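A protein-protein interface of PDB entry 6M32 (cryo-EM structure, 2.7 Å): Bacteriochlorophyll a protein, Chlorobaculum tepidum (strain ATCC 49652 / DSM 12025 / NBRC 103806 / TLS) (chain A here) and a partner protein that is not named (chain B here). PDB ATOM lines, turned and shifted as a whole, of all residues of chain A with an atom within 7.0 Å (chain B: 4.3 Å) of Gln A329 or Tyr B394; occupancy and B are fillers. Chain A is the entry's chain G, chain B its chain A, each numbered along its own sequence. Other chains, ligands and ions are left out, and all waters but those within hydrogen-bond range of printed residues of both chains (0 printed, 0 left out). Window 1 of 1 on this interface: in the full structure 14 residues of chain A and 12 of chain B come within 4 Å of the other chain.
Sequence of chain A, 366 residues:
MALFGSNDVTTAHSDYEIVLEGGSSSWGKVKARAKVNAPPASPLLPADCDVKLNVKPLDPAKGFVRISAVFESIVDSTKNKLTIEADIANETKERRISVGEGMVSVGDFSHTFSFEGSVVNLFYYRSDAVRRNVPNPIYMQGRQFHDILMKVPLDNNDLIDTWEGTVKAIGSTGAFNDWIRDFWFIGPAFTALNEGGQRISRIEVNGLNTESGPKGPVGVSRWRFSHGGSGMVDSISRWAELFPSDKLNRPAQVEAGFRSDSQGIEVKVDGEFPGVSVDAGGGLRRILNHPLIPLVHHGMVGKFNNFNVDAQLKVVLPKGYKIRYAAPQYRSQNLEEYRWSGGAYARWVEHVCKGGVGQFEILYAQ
NH1 of Arg A331 sits at hydrogen-bond distance from O of Asn B272 (3.0 Å). The side-chain amide oxygen (OE1) of Gln A329 sits at hydrogen-bond distance from the backbone NH (N) of Asp B273, at 3.3 Å.
Gln A329 touches Asn B272. OE1 of Gln A329 touches OH of Tyr B394 (3.8 Å). Gln A329 touches Ile B398. Tyr A330 touches Asn B272 (O to O, 3.8 Å). Asn B272 touches Ala A344.
Of the 13 printed residues of chain A, 4 touch a printed residue of chain B. Printed residues of chain A that touch a printed residue of chain B: Gln A329, Tyr A330, Arg A331 and Ala A344. Among the printed residues, 7 pairs touch across the chains. Among the printed residues, no Asp or Glu carboxylate lies within 4 Å of a Lys or Arg side-chain nitrogen of the other chain.
The backbone NH (N) of Arg A331 is in hydrogen-bond range of the backbone carbonyl oxygen (O) of Arg A339. The indole nitrogen (NE1) of Trp A340 lies close to the backbone carbonyl oxygen (O) of Gln A329, at 3.3 Å. O of Ser A341 is in hydrogen-bond range of NE of Arg A331. NZ of Lys B397 is in salt-bridge range of OD2 of Asp B273, 3.5 Å away.
Ala A326 touches none of the printed residues of chain B. Of chain B, only Asn B272, Asp B273, Tyr B394 and Ile B398 come within 4 Å of Gln A329. Of the printed residues of chain B, Tyr A330 touches Asn B272 (3.8 Å). Of the printed residues of chain B, Arg A331 touches Asn B272. Printed residues of chain B within 4 Å of Ala A344: Asn B272 (3.1 Å). Printed residues of chain A within 4 Å of Asp B273: Gln A329. Gln B393 touches none of the printed residues of chain A. Tyr B394 touches one residue of chain A. Of the printed residues of chain A, Ile B398 touches Gln A329 (2.8 Å). The nearest residue of chain B that does not touch Gln A329 is Lys B397 (4.1 Å). The nearest printed residue of chain B that does not touch Ala A344 is Asp B273 (7.8 Å).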
ATOM      1  N   ALA A 326     -14.963 -34.803 -26.647  1.00  0.00           N
ATOM      2  CA  ALA A 326     -15.130 -33.728 -25.678  1.00  0.00           C
ATOM      3  C   ALA A 326     -15.175 -32.411 -26.441  1.00  0.00           C
ATOM      4  O   ALA A 326     -14.205 -32.047 -27.113  1.00  0.00           O
ATOM      5  CB  ALA A 326     -14.002 -33.722 -24.648  1.00  0.00           C
ATOM      6  N   ALA A 327     -16.304 -31.716 -26.361  1.00  0.00           N
ATOM      7  CA  ALA A 327     -16.520 -30.479 -27.111  1.00  0.00           C
ATOM      8  C   ALA A 327     -16.954 -29.369 -26.168  1.00  0.00           C
ATOM      9  O   ALA A 327     -18.091 -29.414 -25.655  1.00  0.00           O
ATOM     10  CB  ALA A 327     -17.570 -30.682 -28.199  1.00  0.00           C
ATOM     11  N   PRO A 328     -16.129 -28.333 -25.940  1.00  0.00           N
ATOM     12  CA  PRO A 328     -14.805 -28.037 -26.500  1.00  0.00           C
ATOM     13  C   PRO A 328     -13.675 -28.939 -26.021  1.00  0.00           C
ATOM     14  O   PRO A 328     -13.845 -29.751 -25.113  1.00  0.00           O
ATOM     15  CB  PRO A 328     -14.546 -26.597 -26.042  1.00  0.00           C
ATOM     16  CG  PRO A 328     -15.441 -26.391 -24.894  1.00  0.00           C
ATOM     17  CD  PRO A 328     -16.661 -27.171 -25.210  1.00  0.00           C
ATOM     18  N   GLN A 329     -12.518 -28.782 -26.653  1.00  0.00           N
ATOM     19  CA  GLN A 329     -11.362 -29.616 -26.381  1.00  0.00           C
ATOM     20  C   GLN A 329     -10.869 -29.411 -24.950  1.00  0.00           C
ATOM     21  O   GLN A 329     -11.071 -28.361 -24.336  1.00  0.00           O
ATOM     22  CB  GLN A 329     -10.248 -29.291 -27.382  1.00  0.00           C
ATOM     23  CG  GLN A 329     -10.408 -29.619 -28.897  1.00  0.00           C
ATOM     24  CD  GLN A 329      -9.281 -29.204 -29.861  1.00  0.00           C
ATOM     25  OE1 GLN A 329      -8.505 -28.277 -29.626  1.00  0.00           O
ATOM     26  NE2 GLN A 329      -9.196 -29.932 -30.969  1.00  0.00           N
ATOM     27  N   TYR A 330     -10.230 -30.447 -24.414  1.00  0.00           N
ATOM     28  CA  TYR A 330      -9.507 -30.331 -23.162  1.00  0.00           C
ATOM     29  C   TYR A 330      -8.083 -29.866 -23.449  1.00  0.00           C
ATOM     30  O   TYR A 330      -7.672 -29.712 -24.600  1.00  0.00           O
ATOM     31  CB  TYR A 330      -9.516 -31.657 -22.404  1.00  0.00           C
ATOM     32  CG  TYR A 330      -9.145 -32.851 -23.249  1.00  0.00           C
ATOM     33  CD1 TYR A 330      -7.832 -33.284 -23.323  1.00  0.00           C
ATOM     34  CD2 TYR A 330     -10.111 -33.570 -23.937  1.00  0.00           C
ATOM     35  CE1 TYR A 330      -7.483 -34.372 -24.089  1.00  0.00           C
ATOM     36  CE2 TYR A 330      -9.772 -34.668 -24.701  1.00  0.00           C
ATOM     37  CZ  TYR A 330      -8.456 -35.063 -24.773  1.00  0.00           C
ATOM     38  OH  TYR A 330      -8.113 -36.156 -25.534  1.00  0.00           O
ATOM     39  N   ARG A 331      -7.317 -29.644 -22.385  1.00  0.00           N
ATOM     40  CA  ARG A 331      -5.956 -29.130 -22.523  1.00  0.00           C
ATOM     41  C   ARG A 331      -4.811 -30.058 -22.117  1.00  0.00           C
ATOM     42  O   ARG A 331      -3.706 -29.939 -22.642  1.00  0.00           O
ATOM     43  CB  ARG A 331      -5.830 -27.830 -21.728  1.00  0.00           C
ATOM     44  CG  ARG A 331      -5.315 -26.651 -22.528  1.00  0.00           C
ATOM     45  CD  ARG A 331      -5.086 -25.450 -21.627  1.00  0.00           C
ATOM     46  NE  ARG A 331      -5.447 -24.203 -22.289  1.00  0.00           N
ATOM     47  CZ  ARG A 331      -5.099 -23.897 -23.532  1.00  0.00           C
ATOM     48  NH1 ARG A 331      -4.377 -24.748 -24.245  1.00  0.00           N
ATOM     49  NH2 ARG A 331      -5.469 -22.739 -24.062  1.00  0.00           N
ATOM     50  N   ARG A 339      -8.068 -31.769 -18.120  1.00  0.00           N
ATOM     51  CA  ARG A 339      -8.195 -30.411 -17.623  1.00  0.00           C
ATOM     52  C   ARG A 339      -8.635 -29.477 -18.739  1.00  0.00           C
ATOM     53  O   ARG A 339      -8.090 -29.507 -19.845  1.00  0.00           O
ATOM     54  CB  ARG A 339      -6.881 -29.928 -17.018  1.00  0.00           C
ATOM     55  CG  ARG A 339      -6.494 -30.687 -15.769  1.00  0.00           C
ATOM     56  CD  ARG A 339      -5.172 -30.216 -15.214  1.00  0.00           C
ATOM     57  NE  ARG A 339      -4.779 -31.004 -14.052  1.00  0.00           N
ATOM     58  CZ  ARG A 339      -4.349 -30.488 -12.906  1.00  0.00           C
ATOM     59  NH1 ARG A 339      -4.247 -29.175 -12.765  1.00  0.00           N
ATOM     60  NH2 ARG A 339      -4.014 -31.289 -11.905  1.00  0.00           N
ATOM     61  N   TRP A 340      -9.629 -28.656 -18.430  1.00  0.00           N
ATOM     62  CA  TRP A 340     -10.145 -27.637 -19.325  1.00  0.00           C
ATOM     63  C   TRP A 340      -9.866 -26.271 -18.719  1.00  0.00           C
ATOM     64  O   TRP A 340     -10.161 -26.038 -17.543  1.00  0.00           O
ATOM     65  CB  TRP A 340     -11.651 -27.790 -19.535  1.00  0.00           C
ATOM     66  CG  TRP A 340     -12.058 -28.943 -20.383  1.00  0.00           C
ATOM     67  CD1 TRP A 340     -12.428 -28.900 -21.689  1.00  0.00           C
ATOM     68  CD2 TRP A 340     -12.178 -30.309 -19.975  1.00  0.00           C
ATOM     69  NE1 TRP A 340     -12.755 -30.156 -22.130  1.00  0.00           N
ATOM     70  CE2 TRP A 340     -12.611 -31.039 -21.095  1.00  0.00           C
ATOM     71  CE3 TRP A 340     -11.952 -30.986 -18.775  1.00  0.00           C
ATOM     72  CZ2 TRP A 340     -12.823 -32.413 -21.052  1.00  0.00           C
ATOM     73  CZ3 TRP A 340     -12.166 -32.347 -18.734  1.00  0.00           C
ATOM     74  CH2 TRP A 340     -12.595 -33.047 -19.865  1.00  0.00           C
ATOM     75  N   SER A 341      -9.311 -25.376 -19.528  1.00  0.00           N
ATOM     76  CA  SER A 341      -9.031 -24.016 -19.093  1.00  0.00           C
ATOM     77  C   SER A 341      -8.899 -23.135 -20.325  1.00  0.00           C
ATOM     78  O   SER A 341      -8.528 -23.603 -21.404  1.00  0.00           O
ATOM     79  CB  SER A 341      -7.761 -23.946 -18.241  1.00  0.00           C
ATOM     80  OG  SER A 341      -7.476 -22.611 -17.865  1.00  0.00           O
ATOM     81  N   GLY A 342      -9.220 -21.858 -20.151  1.00  0.00           N
ATOM     82  CA  GLY A 342      -9.096 -20.874 -21.209  1.00  0.00           C
ATOM     83  C   GLY A 342      -9.836 -21.235 -22.494  1.00  0.00           C
ATOM     84  O   GLY A 342     -10.580 -22.208 -22.584  1.00  0.00           O
ATOM     85  N   ALA A 344     -11.984 -21.902 -25.693  1.00  0.00           N
ATOM     86  CA  ALA A 344     -13.397 -22.185 -25.908  1.00  0.00           C
ATOM     87  C   ALA A 344     -14.092 -22.598 -24.621  1.00  0.00           C
ATOM     88  O   ALA A 344     -15.277 -22.303 -24.442  1.00  0.00           O
ATOM     89  CB  ALA A 344     -13.566 -23.267 -26.970  1.00  0.00           C
ATOM     90  N   TYR A 345     -13.387 -23.281 -23.717  1.00  0.00           N
ATOM     91  CA  TYR A 345     -13.992 -23.606 -22.432  1.00  0.00           C
ATOM     92  C   TYR A 345     -14.288 -22.345 -21.633  1.00  0.00           C
ATOM     93  O   TYR A 345     -15.342 -22.238 -20.998  1.00  0.00           O
ATOM     94  CB  TYR A 345     -13.089 -24.539 -21.631  1.00  0.00           C
ATOM     95  CG  TYR A 345     -13.591 -24.768 -20.227  1.00  0.00           C
ATOM     96  CD1 TYR A 345     -14.667 -25.608 -19.986  1.00  0.00           C
ATOM     97  CD2 TYR A 345     -12.999 -24.141 -19.144  1.00  0.00           C
ATOM     98  CE1 TYR A 345     -15.135 -25.818 -18.711  1.00  0.00           C
ATOM     99  CE2 TYR A 345     -13.461 -24.345 -17.864  1.00  0.00           C
ATOM    100  CZ  TYR A 345     -14.529 -25.185 -17.654  1.00  0.00           C
ATOM    101  OH  TYR A 345     -14.993 -25.394 -16.379  1.00  0.00           O
ATOM    102  N   PHE A 360     -22.197 -28.457 -23.525  1.00  0.00           N
ATOM    103  CA  PHE A 360     -20.824 -28.922 -23.369  1.00  0.00           C
ATOM    104  C   PHE A 360     -20.903 -30.384 -22.948  1.00  0.00           C
ATOM    105  O   PHE A 360     -21.208 -30.686 -21.790  1.00  0.00           O
ATOM    106  CB  PHE A 360     -20.079 -28.072 -22.352  1.00  0.00           C
ATOM    107  CG  PHE A 360     -18.817 -28.693 -21.852  1.00  0.00           C
ATOM    108  CD1 PHE A 360     -17.828 -29.084 -22.725  1.00  0.00           C
ATOM    109  CD2 PHE A 360     -18.620 -28.884 -20.501  1.00  0.00           C
ATOM    110  CE1 PHE A 360     -16.668 -29.653 -22.264  1.00  0.00           C
ATOM    111  CE2 PHE A 360     -17.460 -29.452 -20.035  1.00  0.00           C
ATOM    112  CZ  PHE A 360     -16.484 -29.839 -20.915  1.00  0.00           C
ATOM    113  N   ILE B 269      -8.467 -20.829 -32.874  1.00  0.00           N
ATOM    114  CA  ILE B 269      -8.275 -22.259 -32.663  1.00  0.00           C
ATOM    115  C   ILE B 269      -6.972 -22.573 -31.944  1.00  0.00           C
ATOM    116  O   ILE B 269      -6.801 -23.690 -31.442  1.00  0.00           O
ATOM    117  CB  ILE B 269      -8.331 -22.998 -34.005  1.00  0.00           C
ATOM    118  CG1 ILE B 269      -7.386 -22.343 -35.004  1.00  0.00           C
ATOM    119  CG2 ILE B 269      -9.717 -22.918 -34.561  1.00  0.00           C
ATOM    120  CD1 ILE B 269      -7.155 -23.171 -36.220  1.00  0.00           C
ATOM    121  N   ASN B 272      -7.126 -23.640 -27.707  1.00  0.00           N
ATOM    122  CA  ASN B 272      -7.714 -24.852 -27.142  1.00  0.00           C
ATOM    123  C   ASN B 272      -6.676 -25.954 -26.953  1.00  0.00           C
ATOM    124  O   ASN B 272      -6.350 -26.325 -25.820  1.00  0.00           O
ATOM    125  CB  ASN B 272      -8.851 -25.341 -28.044  1.00  0.00           C
ATOM    126  CG  ASN B 272      -9.925 -24.290 -28.262  1.00  0.00           C
ATOM    127  OD1 ASN B 272      -9.643 -23.102 -28.422  1.00  0.00           O
ATOM    128  ND2 ASN B 272     -11.171 -24.736 -28.282  1.00  0.00           N
ATOM    129  N   ASP B 273      -6.156 -26.497 -28.049  1.00  0.00           N
ATOM    130  CA  ASP B 273      -4.965 -27.347 -27.996  1.00  0.00           C
ATOM    131  C   ASP B 273      -3.735 -26.495 -28.280  1.00  0.00           C
ATOM    132  O   ASP B 273      -3.032 -26.646 -29.279  1.00  0.00           O
ATOM    133  CB  ASP B 273      -5.080 -28.516 -28.970  1.00  0.00           C
ATOM    134  CG  ASP B 273      -3.970 -29.543 -28.776  1.00  0.00           C
ATOM    135  OD1 ASP B 273      -3.356 -29.550 -27.689  1.00  0.00           O
ATOM    136  OD2 ASP B 273      -3.718 -30.351 -29.695  1.00  0.00           O
ATOM    137  N   LYS B 276       0.291 -27.741 -28.880  1.00  0.00           N
ATOM    138  CA  LYS B 276       0.658 -28.388 -30.132  1.00  0.00           C
ATOM    139  C   LYS B 276       0.320 -27.553 -31.354  1.00  0.00           C
ATOM    140  O   LYS B 276       1.134 -27.460 -32.275  1.00  0.00           O
ATOM    141  CB  LYS B 276      -0.031 -29.753 -30.256  1.00  0.00           C
ATOM    142  CG  LYS B 276       0.153 -30.397 -31.624  1.00  0.00           C
ATOM    143  CD  LYS B 276       1.580 -30.832 -31.897  1.00  0.00           C
ATOM    144  CE  LYS B 276       1.915 -32.101 -31.149  1.00  0.00           C
ATOM    145  NZ  LYS B 276       3.310 -32.535 -31.393  1.00  0.00           N
ATOM    146  N   ALA B 277      -0.861 -26.940 -31.388  1.00  0.00           N
ATOM    147  CA  ALA B 277      -1.240 -26.124 -32.536  1.00  0.00           C
ATOM    148  C   ALA B 277      -0.399 -24.856 -32.606  1.00  0.00           C
ATOM    149  O   ALA B 277       0.279 -24.600 -33.607  1.00  0.00           O
ATOM    150  CB  ALA B 277      -2.728 -25.784 -32.469  1.00  0.00           C
ATOM    151  N   HIS B 390       4.200 -31.252 -37.219  1.00  0.00           N
ATOM    152  CA  HIS B 390       3.453 -31.200 -35.968  1.00  0.00           C
ATOM    153  C   HIS B 390       2.078 -30.588 -36.150  1.00  0.00           C
ATOM    154  O   HIS B 390       1.151 -30.931 -35.411  1.00  0.00           O
ATOM    155  CB  HIS B 390       4.235 -30.421 -34.920  1.00  0.00           C
ATOM    156  CG  HIS B 390       5.479 -31.114 -34.480  1.00  0.00           C
ATOM    157  ND1 HIS B 390       6.717 -30.799 -34.989  1.00  0.00           N
ATOM    158  CD2 HIS B 390       5.675 -32.119 -33.597  1.00  0.00           C
ATOM    159  CE1 HIS B 390       7.625 -31.577 -34.432  1.00  0.00           C
ATOM    160  NE2 HIS B 390       7.021 -32.386 -33.583  1.00  0.00           N
ATOM    161  N   GLY B 391       1.930 -29.675 -37.107  1.00  0.00           N
ATOM    162  CA  GLY B 391       0.601 -29.228 -37.474  1.00  0.00           C
ATOM    163  C   GLY B 391      -0.264 -30.366 -37.968  1.00  0.00           C
ATOM    164  O   GLY B 391      -1.464 -30.399 -37.698  1.00  0.00           O
ATOM    165  N   GLY B 392       0.334 -31.314 -38.691  1.00  0.00           N
ATOM    166  CA  GLY B 392      -0.407 -32.484 -39.126  1.00  0.00           C
ATOM    167  C   GLY B 392      -0.809 -33.392 -37.980  1.00  0.00           C
ATOM    168  O   GLY B 392      -1.890 -33.986 -38.003  1.00  0.00           O
ATOM    169  N   GLN B 393       0.064 -33.538 -36.980  1.00  0.00           N
ATOM    170  CA  GLN B 393      -0.278 -34.356 -35.822  1.00  0.00           C
ATOM    171  C   GLN B 393      -1.489 -33.786 -35.103  1.00  0.00           C
ATOM    172  O   GLN B 393      -2.409 -34.523 -34.733  1.00  0.00           O
ATOM    173  CB  GLN B 393       0.916 -34.453 -34.877  1.00  0.00           C
ATOM    174  CG  GLN B 393       1.980 -35.416 -35.338  1.00  0.00           C
ATOM    175  CD  GLN B 393       3.160 -35.458 -34.399  1.00  0.00           C
ATOM    176  OE1 GLN B 393       3.504 -34.458 -33.773  1.00  0.00           O
ATOM    177  NE2 GLN B 393       3.781 -36.621 -34.286  1.00  0.00           N
ATOM    178  N   TYR B 394      -1.510 -32.470 -34.908  1.00  0.00           N
ATOM    179  CA  TYR B 394      -2.721 -31.814 -34.436  1.00  0.00           C
ATOM    180  C   TYR B 394      -3.853 -31.933 -35.445  1.00  0.00           C
ATOM    181  O   TYR B 394      -4.993 -32.225 -35.071  1.00  0.00           O
ATOM    182  CB  TYR B 394      -2.439 -30.350 -34.126  1.00  0.00           C
ATOM    183  CG  TYR B 394      -3.689 -29.557 -33.843  1.00  0.00           C
ATOM    184  CD1 TYR B 394      -4.279 -29.584 -32.594  1.00  0.00           C
ATOM    185  CD2 TYR B 394      -4.269 -28.768 -34.826  1.00  0.00           C
ATOM    186  CE1 TYR B 394      -5.421 -28.866 -32.335  1.00  0.00           C
ATOM    187  CE2 TYR B 394      -5.411 -28.042 -34.572  1.00  0.00           C
ATOM    188  CZ  TYR B 394      -5.981 -28.094 -33.324  1.00  0.00           C
ATOM    189  OH  TYR B 394      -7.118 -27.371 -33.061  1.00  0.00           O
ATOM    190  N   LEU B 395      -3.564 -31.706 -36.725  1.00  0.00           N
ATOM    191  CA  LEU B 395      -4.629 -31.683 -37.722  1.00  0.00           C
ATOM    192  C   LEU B 395      -5.320 -33.039 -37.807  1.00  0.00           C
ATOM    193  O   LEU B 395      -6.545 -33.118 -37.943  1.00  0.00           O
ATOM    194  CB  LEU B 395      -4.062 -31.268 -39.080  1.00  0.00           C
ATOM    195  CG  LEU B 395      -4.771 -30.101 -39.765  1.00  0.00           C
ATOM    196  CD1 LEU B 395      -4.555 -28.819 -38.972  1.00  0.00           C
ATOM    197  CD2 LEU B 395      -4.267 -29.939 -41.183  1.00  0.00           C
ATOM    198  N   LEU B 396      -4.547 -34.122 -37.713  1.00  0.00           N
ATOM    199  CA  LEU B 396      -5.139 -35.454 -37.690  1.00  0.00           C
ATOM    200  C   LEU B 396      -6.008 -35.663 -36.457  1.00  0.00           C
ATOM    201  O   LEU B 396      -7.079 -36.273 -36.548  1.00  0.00           O
ATOM    202  CB  LEU B 396      -4.039 -36.511 -37.734  1.00  0.00           C
ATOM    203  CG  LEU B 396      -4.551 -37.947 -37.761  1.00  0.00           C
ATOM    204  CD1 LEU B 396      -5.355 -38.173 -39.017  1.00  0.00           C
ATOM    205  CD2 LEU B 396      -3.428 -38.948 -37.669  1.00  0.00           C
ATOM    206  N   LYS B 397      -5.564 -35.167 -35.301  1.00  0.00           N
ATOM    207  CA  LYS B 397      -6.265 -35.434 -34.049  1.00  0.00           C
ATOM    208  C   LYS B 397      -7.662 -34.823 -34.047  1.00  0.00           C
ATOM    209  O   LYS B 397      -8.623 -35.452 -33.594  1.00  0.00           O
ATOM    210  CB  LYS B 397      -5.442 -34.910 -32.874  1.00  0.00           C
ATOM    211  CG  LYS B 397      -6.063 -35.184 -31.525  1.00  0.00           C
ATOM    212  CD  LYS B 397      -5.145 -34.765 -30.399  1.00  0.00           C
ATOM    213  CE  LYS B 397      -5.054 -33.255 -30.304  1.00  0.00           C
ATOM    214  NZ  LYS B 397      -6.338 -32.644 -29.864  1.00  0.00           N
ATOM    215  N   ILE B 398      -7.799 -33.596 -34.552  1.00  0.00           N
ATOM    216  CA  ILE B 398      -9.112 -32.963 -34.574  1.00  0.00           C
ATOM    217  C   ILE B 398     -10.036 -33.568 -35.615  1.00  0.00           C
ATOM    218  O   ILE B 398     -11.236 -33.274 -35.605  1.00  0.00           O
ATOM    219  CB  ILE B 398      -9.002 -31.443 -34.807  1.00  0.00           C
ATOM    220  CG1 ILE B 398      -8.156 -31.145 -36.041  1.00  0.00           C
ATOM    221  CG2 ILE B 398      -8.424 -30.758 -33.583  1.00  0.00           C
ATOM    222  CD1 ILE B 398      -8.222 -29.707 -36.481  1.00  0.00           C
